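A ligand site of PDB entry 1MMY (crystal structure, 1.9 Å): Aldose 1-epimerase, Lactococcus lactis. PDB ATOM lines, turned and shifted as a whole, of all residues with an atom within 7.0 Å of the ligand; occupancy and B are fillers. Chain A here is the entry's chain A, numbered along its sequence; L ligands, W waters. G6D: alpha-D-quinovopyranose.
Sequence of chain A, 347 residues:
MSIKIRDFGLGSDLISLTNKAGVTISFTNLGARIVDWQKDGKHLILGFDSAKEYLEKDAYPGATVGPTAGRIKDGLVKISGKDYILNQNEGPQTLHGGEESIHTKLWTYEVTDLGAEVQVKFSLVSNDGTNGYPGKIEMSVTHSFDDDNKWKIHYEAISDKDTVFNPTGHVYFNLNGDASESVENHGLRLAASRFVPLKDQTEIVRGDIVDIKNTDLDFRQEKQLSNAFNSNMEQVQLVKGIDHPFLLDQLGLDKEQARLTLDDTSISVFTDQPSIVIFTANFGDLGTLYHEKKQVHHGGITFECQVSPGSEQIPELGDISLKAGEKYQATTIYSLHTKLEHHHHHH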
ATOM      1  N   ASP A  58      17.222 -27.275 -17.577  1.00  0.00           N
ATOM      2  CA  ASP A  58      17.027 -26.053 -16.868  1.00  0.00           C
ATOM      3  C   ASP A  58      16.824 -26.494 -15.446  1.00  0.00           C
ATOM      4  O   ASP A  58      15.866 -27.240 -15.222  1.00  0.00           O
ATOM      5  CB  ASP A  58      15.848 -25.213 -17.406  1.00  0.00           C
ATOM      6  CG  ASP A  58      15.720 -23.937 -16.593  1.00  0.00           C
ATOM      7  OD1 ASP A  58      16.492 -23.608 -15.721  1.00  0.00           O
ATOM      8  OD2 ASP A  58      14.718 -23.177 -16.935  1.00  0.00           O
ATOM      9  N   TYR A  60      16.241 -24.579 -12.792  1.00  0.00           N
ATOM     10  CA  TYR A  60      15.417 -23.726 -11.922  1.00  0.00           C
ATOM     11  C   TYR A  60      13.951 -24.028 -11.730  1.00  0.00           C
ATOM     12  O   TYR A  60      13.402 -23.800 -10.628  1.00  0.00           O
ATOM     13  CB  TYR A  60      15.537 -22.259 -12.340  1.00  0.00           C
ATOM     14  CG  TYR A  60      16.932 -21.726 -12.065  1.00  0.00           C
ATOM     15  CD1 TYR A  60      17.755 -21.303 -13.111  1.00  0.00           C
ATOM     16  CD2 TYR A  60      17.459 -21.670 -10.780  1.00  0.00           C
ATOM     17  CE1 TYR A  60      19.039 -20.799 -12.881  1.00  0.00           C
ATOM     18  CE2 TYR A  60      18.739 -21.165 -10.541  1.00  0.00           C
ATOM     19  CZ  TYR A  60      19.538 -20.724 -11.587  1.00  0.00           C
ATOM     20  OH  TYR A  60      20.792 -20.222 -11.361  1.00  0.00           O
ATOM     21  N   VAL A  65      15.274 -21.866  -4.519  1.00  0.00           N
ATOM     22  CA  VAL A  65      16.508 -21.209  -4.900  1.00  0.00           C
ATOM     23  C   VAL A  65      16.933 -20.326  -3.728  1.00  0.00           C
ATOM     24  O   VAL A  65      16.104 -19.814  -2.976  1.00  0.00           O
ATOM     25  CB  VAL A  65      16.496 -20.364  -6.175  1.00  0.00           C
ATOM     26  CG1 VAL A  65      16.109 -21.213  -7.383  1.00  0.00           C
ATOM     27  CG2 VAL A  65      15.455 -19.281  -5.995  1.00  0.00           C
ATOM     28  N   GLY A  70      17.366 -14.277  -6.693  1.00  0.00           N
ATOM     29  CA  GLY A  70      17.496 -13.056  -7.455  1.00  0.00           C
ATOM     30  C   GLY A  70      18.924 -12.665  -7.784  1.00  0.00           C
ATOM     31  O   GLY A  70      19.856 -13.431  -7.523  1.00  0.00           O
ATOM     32  N   ARG A  71      19.091 -11.464  -8.371  1.00  0.00           N
ATOM     33  CA  ARG A  71      20.415 -10.920  -8.713  1.00  0.00           C
ATOM     34  C   ARG A  71      21.000  -9.954  -7.692  1.00  0.00           C
ATOM     35  O   ARG A  71      20.309  -8.997  -7.254  1.00  0.00           O
ATOM     36  CB  ARG A  71      20.386 -10.077  -9.975  1.00  0.00           C
ATOM     37  CG  ARG A  71      19.948 -10.920 -11.129  1.00  0.00           C
ATOM     38  CD  ARG A  71      19.900 -10.178 -12.472  1.00  0.00           C
ATOM     39  NE  ARG A  71      19.872 -11.213 -13.520  1.00  0.00           N
ATOM     40  CZ  ARG A  71      18.780 -11.842 -13.961  1.00  0.00           C
ATOM     41  NH1 ARG A  71      17.525 -11.559 -13.535  1.00  0.00           N
ATOM     42  NH2 ARG A  71      18.982 -12.770 -14.879  1.00  0.00           N
ATOM     43  N   GLU A  90      26.770 -14.892 -13.255  1.00  0.00           N
ATOM     44  CA  GLU A  90      26.118 -14.308 -14.381  1.00  0.00           C
ATOM     45  C   GLU A  90      26.834 -13.019 -14.577  1.00  0.00           C
ATOM     46  O   GLU A  90      26.419 -11.982 -14.053  1.00  0.00           O
ATOM     47  CB  GLU A  90      24.666 -14.028 -14.075  1.00  0.00           C
ATOM     48  CG  GLU A  90      23.998 -13.514 -15.337  1.00  0.00           C
ATOM     49  CD  GLU A  90      22.608 -12.989 -15.056  1.00  0.00           C
ATOM     50  OE1 GLU A  90      22.395 -12.069 -14.313  1.00  0.00           O
ATOM     51  OE2 GLU A  90      21.654 -13.645 -15.676  1.00  0.00           O
ATOM     52  N   LEU A  95      23.556 -14.662  -9.199  1.00  0.00           N
ATOM     53  CA  LEU A  95      22.150 -14.924  -9.490  1.00  0.00           C
ATOM     54  C   LEU A  95      21.689 -16.209  -8.819  1.00  0.00           C
ATOM     55  O   LEU A  95      22.308 -17.224  -8.994  1.00  0.00           O
ATOM     56  CB  LEU A  95      21.948 -15.054 -11.008  1.00  0.00           C
ATOM     57  CG  LEU A  95      20.607 -15.712 -11.374  1.00  0.00           C
ATOM     58  CD1 LEU A  95      19.439 -14.718 -11.262  1.00  0.00           C
ATOM     59  CD2 LEU A  95      20.703 -16.303 -12.752  1.00  0.00           C
ATOM     60  N   HIS A  96      20.625 -16.156  -8.051  1.00  0.00           N
ATOM     61  CA  HIS A  96      20.108 -17.355  -7.370  1.00  0.00           C
ATOM     62  C   HIS A  96      21.120 -18.140  -6.532  1.00  0.00           C
ATOM     63  O   HIS A  96      21.139 -19.402  -6.571  1.00  0.00           O
ATOM     64  CB  HIS A  96      19.355 -18.294  -8.351  1.00  0.00           C
ATOM     65  CG  HIS A  96      18.167 -17.624  -9.003  1.00  0.00           C
ATOM     66  ND1 HIS A  96      17.405 -16.624  -8.363  1.00  0.00           N
ATOM     67  CD2 HIS A  96      17.665 -17.839 -10.227  1.00  0.00           C
ATOM     68  CE1 HIS A  96      16.474 -16.264  -9.215  1.00  0.00           C
ATOM     69  NE2 HIS A  96      16.592 -16.976 -10.353  1.00  0.00           N
ATOM     70  N   HIS A 170      10.664 -21.442  -7.185  1.00  0.00           N
ATOM     71  CA  HIS A 170      10.642 -21.058  -8.577  1.00  0.00           C
ATOM     72  C   HIS A 170       9.693 -21.842  -9.503  1.00  0.00           C
ATOM     73  O   HIS A 170      10.030 -22.116 -10.668  1.00  0.00           O
ATOM     74  CB  HIS A 170      12.092 -21.125  -9.108  1.00  0.00           C
ATOM     75  CG  HIS A 170      12.404 -20.108 -10.202  1.00  0.00           C
ATOM     76  ND1 HIS A 170      12.021 -20.293 -11.555  1.00  0.00           N
ATOM     77  CD2 HIS A 170      13.084 -18.945 -10.131  1.00  0.00           C
ATOM     78  CE1 HIS A 170      12.477 -19.230 -12.228  1.00  0.00           C
ATOM     79  NE2 HIS A 170      13.117 -18.398 -11.409  1.00  0.00           N
ATOM     80  N   TYR A 172       6.844 -22.529 -12.169  1.00  0.00           N
ATOM     81  CA  TYR A 172       6.309 -21.826 -13.321  1.00  0.00           C
ATOM     82  C   TYR A 172       4.907 -22.439 -13.571  1.00  0.00           C
ATOM     83  O   TYR A 172       4.734 -23.665 -13.682  1.00  0.00           O
ATOM     84  CB  TYR A 172       7.072 -22.096 -14.620  1.00  0.00           C
ATOM     85  CG  TYR A 172       8.396 -21.394 -14.831  1.00  0.00           C
ATOM     86  CD1 TYR A 172       9.594 -22.069 -14.577  1.00  0.00           C
ATOM     87  CD2 TYR A 172       8.469 -20.129 -15.395  1.00  0.00           C
ATOM     88  CE1 TYR A 172      10.839 -21.492 -14.811  1.00  0.00           C
ATOM     89  CE2 TYR A 172       9.707 -19.533 -15.642  1.00  0.00           C
ATOM     90  CZ  TYR A 172      10.884 -20.220 -15.366  1.00  0.00           C
ATOM     91  OH  TYR A 172      12.132 -19.632 -15.609  1.00  0.00           O
ATOM     92  N   GLU A 203      19.883  -6.674 -16.019  1.00  0.00           N
ATOM     93  CA  GLU A 203      18.793  -6.935 -15.110  1.00  0.00           C
ATOM     94  C   GLU A 203      19.019  -6.572 -13.671  1.00  0.00           C
ATOM     95  O   GLU A 203      18.291  -7.006 -12.790  1.00  0.00           O
ATOM     96  CB  GLU A 203      18.190  -8.342 -15.322  1.00  0.00           C
ATOM     97  CG  GLU A 203      17.527  -8.508 -16.702  1.00  0.00           C
ATOM     98  CD  GLU A 203      17.471  -9.900 -17.333  1.00  0.00           C
ATOM     99  OE1 GLU A 203      18.386 -10.427 -17.964  1.00  0.00           O
ATOM    100  OE2 GLU A 203      16.300 -10.440 -17.228  1.00  0.00           O
ATOM    101  N   VAL A 239      12.812  -6.386 -21.377  1.00  0.00           N
ATOM    102  CA  VAL A 239      12.925  -7.834 -21.132  1.00  0.00           C
ATOM    103  C   VAL A 239      12.067  -8.702 -22.050  1.00  0.00           C
ATOM    104  O   VAL A 239      12.224  -9.954 -22.031  1.00  0.00           O
ATOM    105  CB  VAL A 239      12.748  -8.213 -19.660  1.00  0.00           C
ATOM    106  CG1 VAL A 239      13.804  -7.532 -18.776  1.00  0.00           C
ATOM    107  CG2 VAL A 239      11.355  -7.882 -19.144  1.00  0.00           C
ATOM    108  N   ASP A 243       9.753  -9.337 -15.963  1.00  0.00           N
ATOM    109  CA  ASP A 243      10.880  -9.902 -15.225  1.00  0.00           C
ATOM    110  C   ASP A 243      11.197  -8.896 -14.146  1.00  0.00           C
ATOM    111  O   ASP A 243      12.241  -8.287 -14.188  1.00  0.00           O
ATOM    112  CB  ASP A 243      12.120 -10.162 -16.094  1.00  0.00           C
ATOM    113  CG  ASP A 243      13.023 -11.214 -15.469  1.00  0.00           C
ATOM    114  OD1 ASP A 243      12.870 -11.658 -14.346  1.00  0.00           O
ATOM    115  OD2 ASP A 243      13.914 -11.660 -16.309  1.00  0.00           O
ATOM    116  N   HIS A 244      10.246  -8.736 -13.215  1.00  0.00           N
ATOM    117  CA  HIS A 244      10.349  -7.736 -12.198  1.00  0.00           C
ATOM    118  C   HIS A 244       9.689  -8.059 -10.887  1.00  0.00           C
ATOM    119  O   HIS A 244       8.757  -8.852 -10.798  1.00  0.00           O
ATOM    120  CB  HIS A 244       9.502  -6.531 -12.688  1.00  0.00           C
ATOM    121  CG  HIS A 244      10.037  -5.917 -13.947  1.00  0.00           C
ATOM    122  ND1 HIS A 244       9.817  -6.482 -15.214  1.00  0.00           N
ATOM    123  CD2 HIS A 244      10.777  -4.777 -14.104  1.00  0.00           C
ATOM    124  CE1 HIS A 244      10.446  -5.704 -16.104  1.00  0.00           C
ATOM    125  NE2 HIS A 244      11.001  -4.676 -15.454  1.00  0.00           N
ATOM    126  N   VAL A 277       8.080 -11.525  -7.302  1.00  0.00           N
ATOM    127  CA  VAL A 277       8.843 -11.386  -8.503  1.00  0.00           C
ATOM    128  C   VAL A 277       8.150 -12.229  -9.572  1.00  0.00           C
ATOM    129  O   VAL A 277       7.886 -13.434  -9.392  1.00  0.00           O
ATOM    130  CB  VAL A 277      10.306 -11.770  -8.281  1.00  0.00           C
ATOM    131  CG1 VAL A 277      11.053 -11.641  -9.625  1.00  0.00           C
ATOM    132  CG2 VAL A 277      10.944 -10.851  -7.225  1.00  0.00           C
ATOM    133  N   ILE A 278       7.820 -11.571 -10.679  1.00  0.00           N
ATOM    134  CA  ILE A 278       7.145 -12.222 -11.787  1.00  0.00           C
ATOM    135  C   ILE A 278       8.008 -12.285 -13.025  1.00  0.00           C
ATOM    136  O   ILE A 278       8.505 -11.290 -13.525  1.00  0.00           O
ATOM    137  CB  ILE A 278       5.832 -11.514 -12.130  1.00  0.00           C
ATOM    138  CG1 ILE A 278       4.942 -11.513 -10.897  1.00  0.00           C
ATOM    139  CG2 ILE A 278       5.110 -12.198 -13.296  1.00  0.00           C
ATOM    140  CD1 ILE A 278       3.629 -10.806 -11.106  1.00  0.00           C
ATOM    141  N   PHE A 279       8.161 -13.482 -13.498  1.00  0.00           N
ATOM    142  CA  PHE A 279       8.951 -13.702 -14.703  1.00  0.00           C
ATOM    143  C   PHE A 279       8.072 -14.510 -15.651  1.00  0.00           C
ATOM    144  O   PHE A 279       7.481 -15.551 -15.269  1.00  0.00           O
ATOM    145  CB  PHE A 279      10.285 -14.398 -14.337  1.00  0.00           C
ATOM    146  CG  PHE A 279      11.072 -14.939 -15.513  1.00  0.00           C
ATOM    147  CD1 PHE A 279      11.523 -14.043 -16.488  1.00  0.00           C
ATOM    148  CD2 PHE A 279      11.336 -16.302 -15.648  1.00  0.00           C
ATOM    149  CE1 PHE A 279      12.268 -14.508 -17.569  1.00  0.00           C
ATOM    150  CE2 PHE A 279      12.061 -16.788 -16.730  1.00  0.00           C
ATOM    151  CZ  PHE A 279      12.550 -15.870 -17.672  1.00  0.00           C
ATOM    152  N   ASN A 282      10.518 -15.369 -20.747  1.00  0.00           N
ATOM    153  CA  ASN A 282      10.842 -14.631 -21.937  1.00  0.00           C
ATOM    154  C   ASN A 282      12.016 -15.268 -22.667  1.00  0.00           C
ATOM    155  O   ASN A 282      13.004 -14.609 -22.959  1.00  0.00           O
ATOM    156  CB  ASN A 282      11.173 -13.187 -21.457  1.00  0.00           C
ATOM    157  CG  ASN A 282      10.103 -12.644 -20.522  1.00  0.00           C
ATOM    158  OD1 ASN A 282       8.902 -12.893 -20.687  1.00  0.00           O
ATOM    159  ND2 ASN A 282      10.517 -11.841 -19.539  1.00  0.00           N
ATOM    160  N   PHE A 283      11.911 -16.556 -22.993  1.00  0.00           N
ATOM    161  CA  PHE A 283      13.021 -17.229 -23.634  1.00  0.00           C
ATOM    162  C   PHE A 283      13.153 -17.154 -25.131  1.00  0.00           C
ATOM    163  O   PHE A 283      14.073 -17.751 -25.718  1.00  0.00           O
ATOM    164  CB  PHE A 283      13.113 -18.710 -23.233  1.00  0.00           C
ATOM    165  CG  PHE A 283      13.100 -18.877 -21.736  1.00  0.00           C
ATOM    166  CD1 PHE A 283      12.023 -19.475 -21.073  1.00  0.00           C
ATOM    167  CD2 PHE A 283      14.179 -18.453 -20.953  1.00  0.00           C
ATOM    168  CE1 PHE A 283      12.011 -19.651 -19.688  1.00  0.00           C
ATOM    169  CE2 PHE A 283      14.189 -18.616 -19.568  1.00  0.00           C
ATOM    170  CZ  PHE A 283      13.103 -19.216 -18.931  1.00  0.00           C
ATOM    171  N   THR A 302       5.993 -17.116 -13.301  1.00  0.00           N
ATOM    172  CA  THR A 302       6.330 -17.406 -11.926  1.00  0.00           C
ATOM    173  C   THR A 302       5.708 -16.419 -10.959  1.00  0.00           C
ATOM    174  O   THR A 302       5.339 -15.320 -11.315  1.00  0.00           O
ATOM    175  CB  THR A 302       7.892 -17.301 -11.677  1.00  0.00           C
ATOM    176  OG1 THR A 302       8.306 -15.945 -11.797  1.00  0.00           O
ATOM    177  CG2 THR A 302       8.838 -18.124 -12.552  1.00  0.00           C
ATOM    178  N   GLU A 304       7.407 -15.534  -7.572  1.00  0.00           N
ATOM    179  CA  GLU A 304       8.479 -15.745  -6.575  1.00  0.00           C
ATOM    180  C   GLU A 304       8.271 -14.799  -5.403  1.00  0.00           C
ATOM    181  O   GLU A 304       8.552 -13.624  -5.498  1.00  0.00           O
ATOM    182  CB  GLU A 304       9.819 -15.477  -7.246  1.00  0.00           C
ATOM    183  CG  GLU A 304      10.035 -16.482  -8.406  1.00  0.00           C
ATOM    184  CD  GLU A 304      11.214 -16.145  -9.278  1.00  0.00           C
ATOM    185  OE1 GLU A 304      12.346 -16.125  -8.856  1.00  0.00           O
ATOM    186  OE2 GLU A 304      10.921 -15.853 -10.518  1.00  0.00           O
ATOM    187  N   PRO A 309      14.560  -8.228  -4.788  1.00  0.00           N
ATOM    188  CA  PRO A 309      15.983  -8.119  -5.067  1.00  0.00           C
ATOM    189  C   PRO A 309      16.335  -6.637  -5.190  1.00  0.00           C
ATOM    190  O   PRO A 309      15.458  -5.828  -5.433  1.00  0.00           O
ATOM    191  CB  PRO A 309      16.174  -8.722  -6.477  1.00  0.00           C
ATOM    192  CG  PRO A 309      14.827  -9.229  -6.962  1.00  0.00           C
ATOM    193  CD  PRO A 309      13.833  -9.034  -5.817  1.00  0.00           C
HETATM  194  C1  G6D L   1      15.521 -14.155 -15.545  1.00  0.00           C
HETATM  195  O2  G6D L   1      16.504 -16.178 -16.526  1.00  0.00           O
HETATM  196  C2  G6D L   1      16.171 -15.533 -15.330  1.00  0.00           C
HETATM  197  C3  G6D L   1      15.224 -16.384 -14.490  1.00  0.00           C
HETATM  198  O3  G6D L   1      15.548 -17.786 -14.339  1.00  0.00           O
HETATM  199  C4  G6D L   1      15.183 -15.699 -13.168  1.00  0.00           C
HETATM  200  O4  G6D L   1      14.423 -16.466 -12.265  1.00  0.00           O
HETATM  201  C5  G6D L   1      14.496 -14.353 -13.482  1.00  0.00           C
HETATM  202  O5  G6D L   1      15.287 -13.513 -14.300  1.00  0.00           O
HETATM  203  C6  G6D L   1      14.057 -13.485 -12.329  1.00  0.00           C
HETATM  204  O1  G6D L   1      16.332 -13.284 -16.340  1.00  0.00           O
HETATM  205  O   HOH W   1      14.845 -12.337  -9.910  1.00  0.00           O
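NE2 of His 170 is in hydrogen-bond range of OE2 of Glu 304, at 3.5 Å. N of Asp 243 lies close to O of Ile 278, 3.4 Å away. The backbone NH of His 96 is in hydrogen-bond range of the backbone carbonyl oxygen of Gly 70 (2.9 Å). The side-chain carboxylate (OE1) of Glu 203 lies within salt-bridge range of the guanidinium group (NH2) of Arg 71, 3.9 Å away. OE1 of Glu 90 lies within salt-bridge range of NE of Arg 71, at 2.8 Å. The backbone NH of Thr 302 lies within hydrogen-bond range of the backbone carbonyl oxygen of Phe 279 (2.9 Å). The backbone carbonyl oxygen of Glu 304 sits at hydrogen-bond distance from the backbone NH of Val 277 (2.8 Å). OG1 of Thr 302 is in hydrogen-bond range of OE2 of Glu 304, 2.9 Å away.
Phe 279 touches the ligand. Glu 304 touches the ligand (OE2 to O4, 3.96 Å). Hydrophobic or aromatic side chains within 4 Å of the ligand: His 96, His 170 and Phe 279. Seven residues have an atom within 4 Å of the ligand: Arg 71, His 96, His 170, Glu 203, Asp 243, Phe 279 and Glu 304. The nearest printed residue that does not touch the ligand is Tyr 172 (4.1 Å).
NE2 of His 170 sits at hydrogen-bond distance from O4 of the ligand. The side-chain carboxylate (OD2) of Asp 243 lies within hydrogen-bond range of an oxygen (O1) of the ligand (2.9 Å). A ring nitrogen (NE2) of His 96 lies within hydrogen-bond range of an oxygen (O4) of the ligand (2.9 Å). An oxygen (O1) of the ligand is in hydrogen-bond range of the side-chain carboxylate (OE2) of Glu 203. O5 of the ligand sits at hydrogen-bond distance from NH1 of Arg 71 (3.1 Å).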
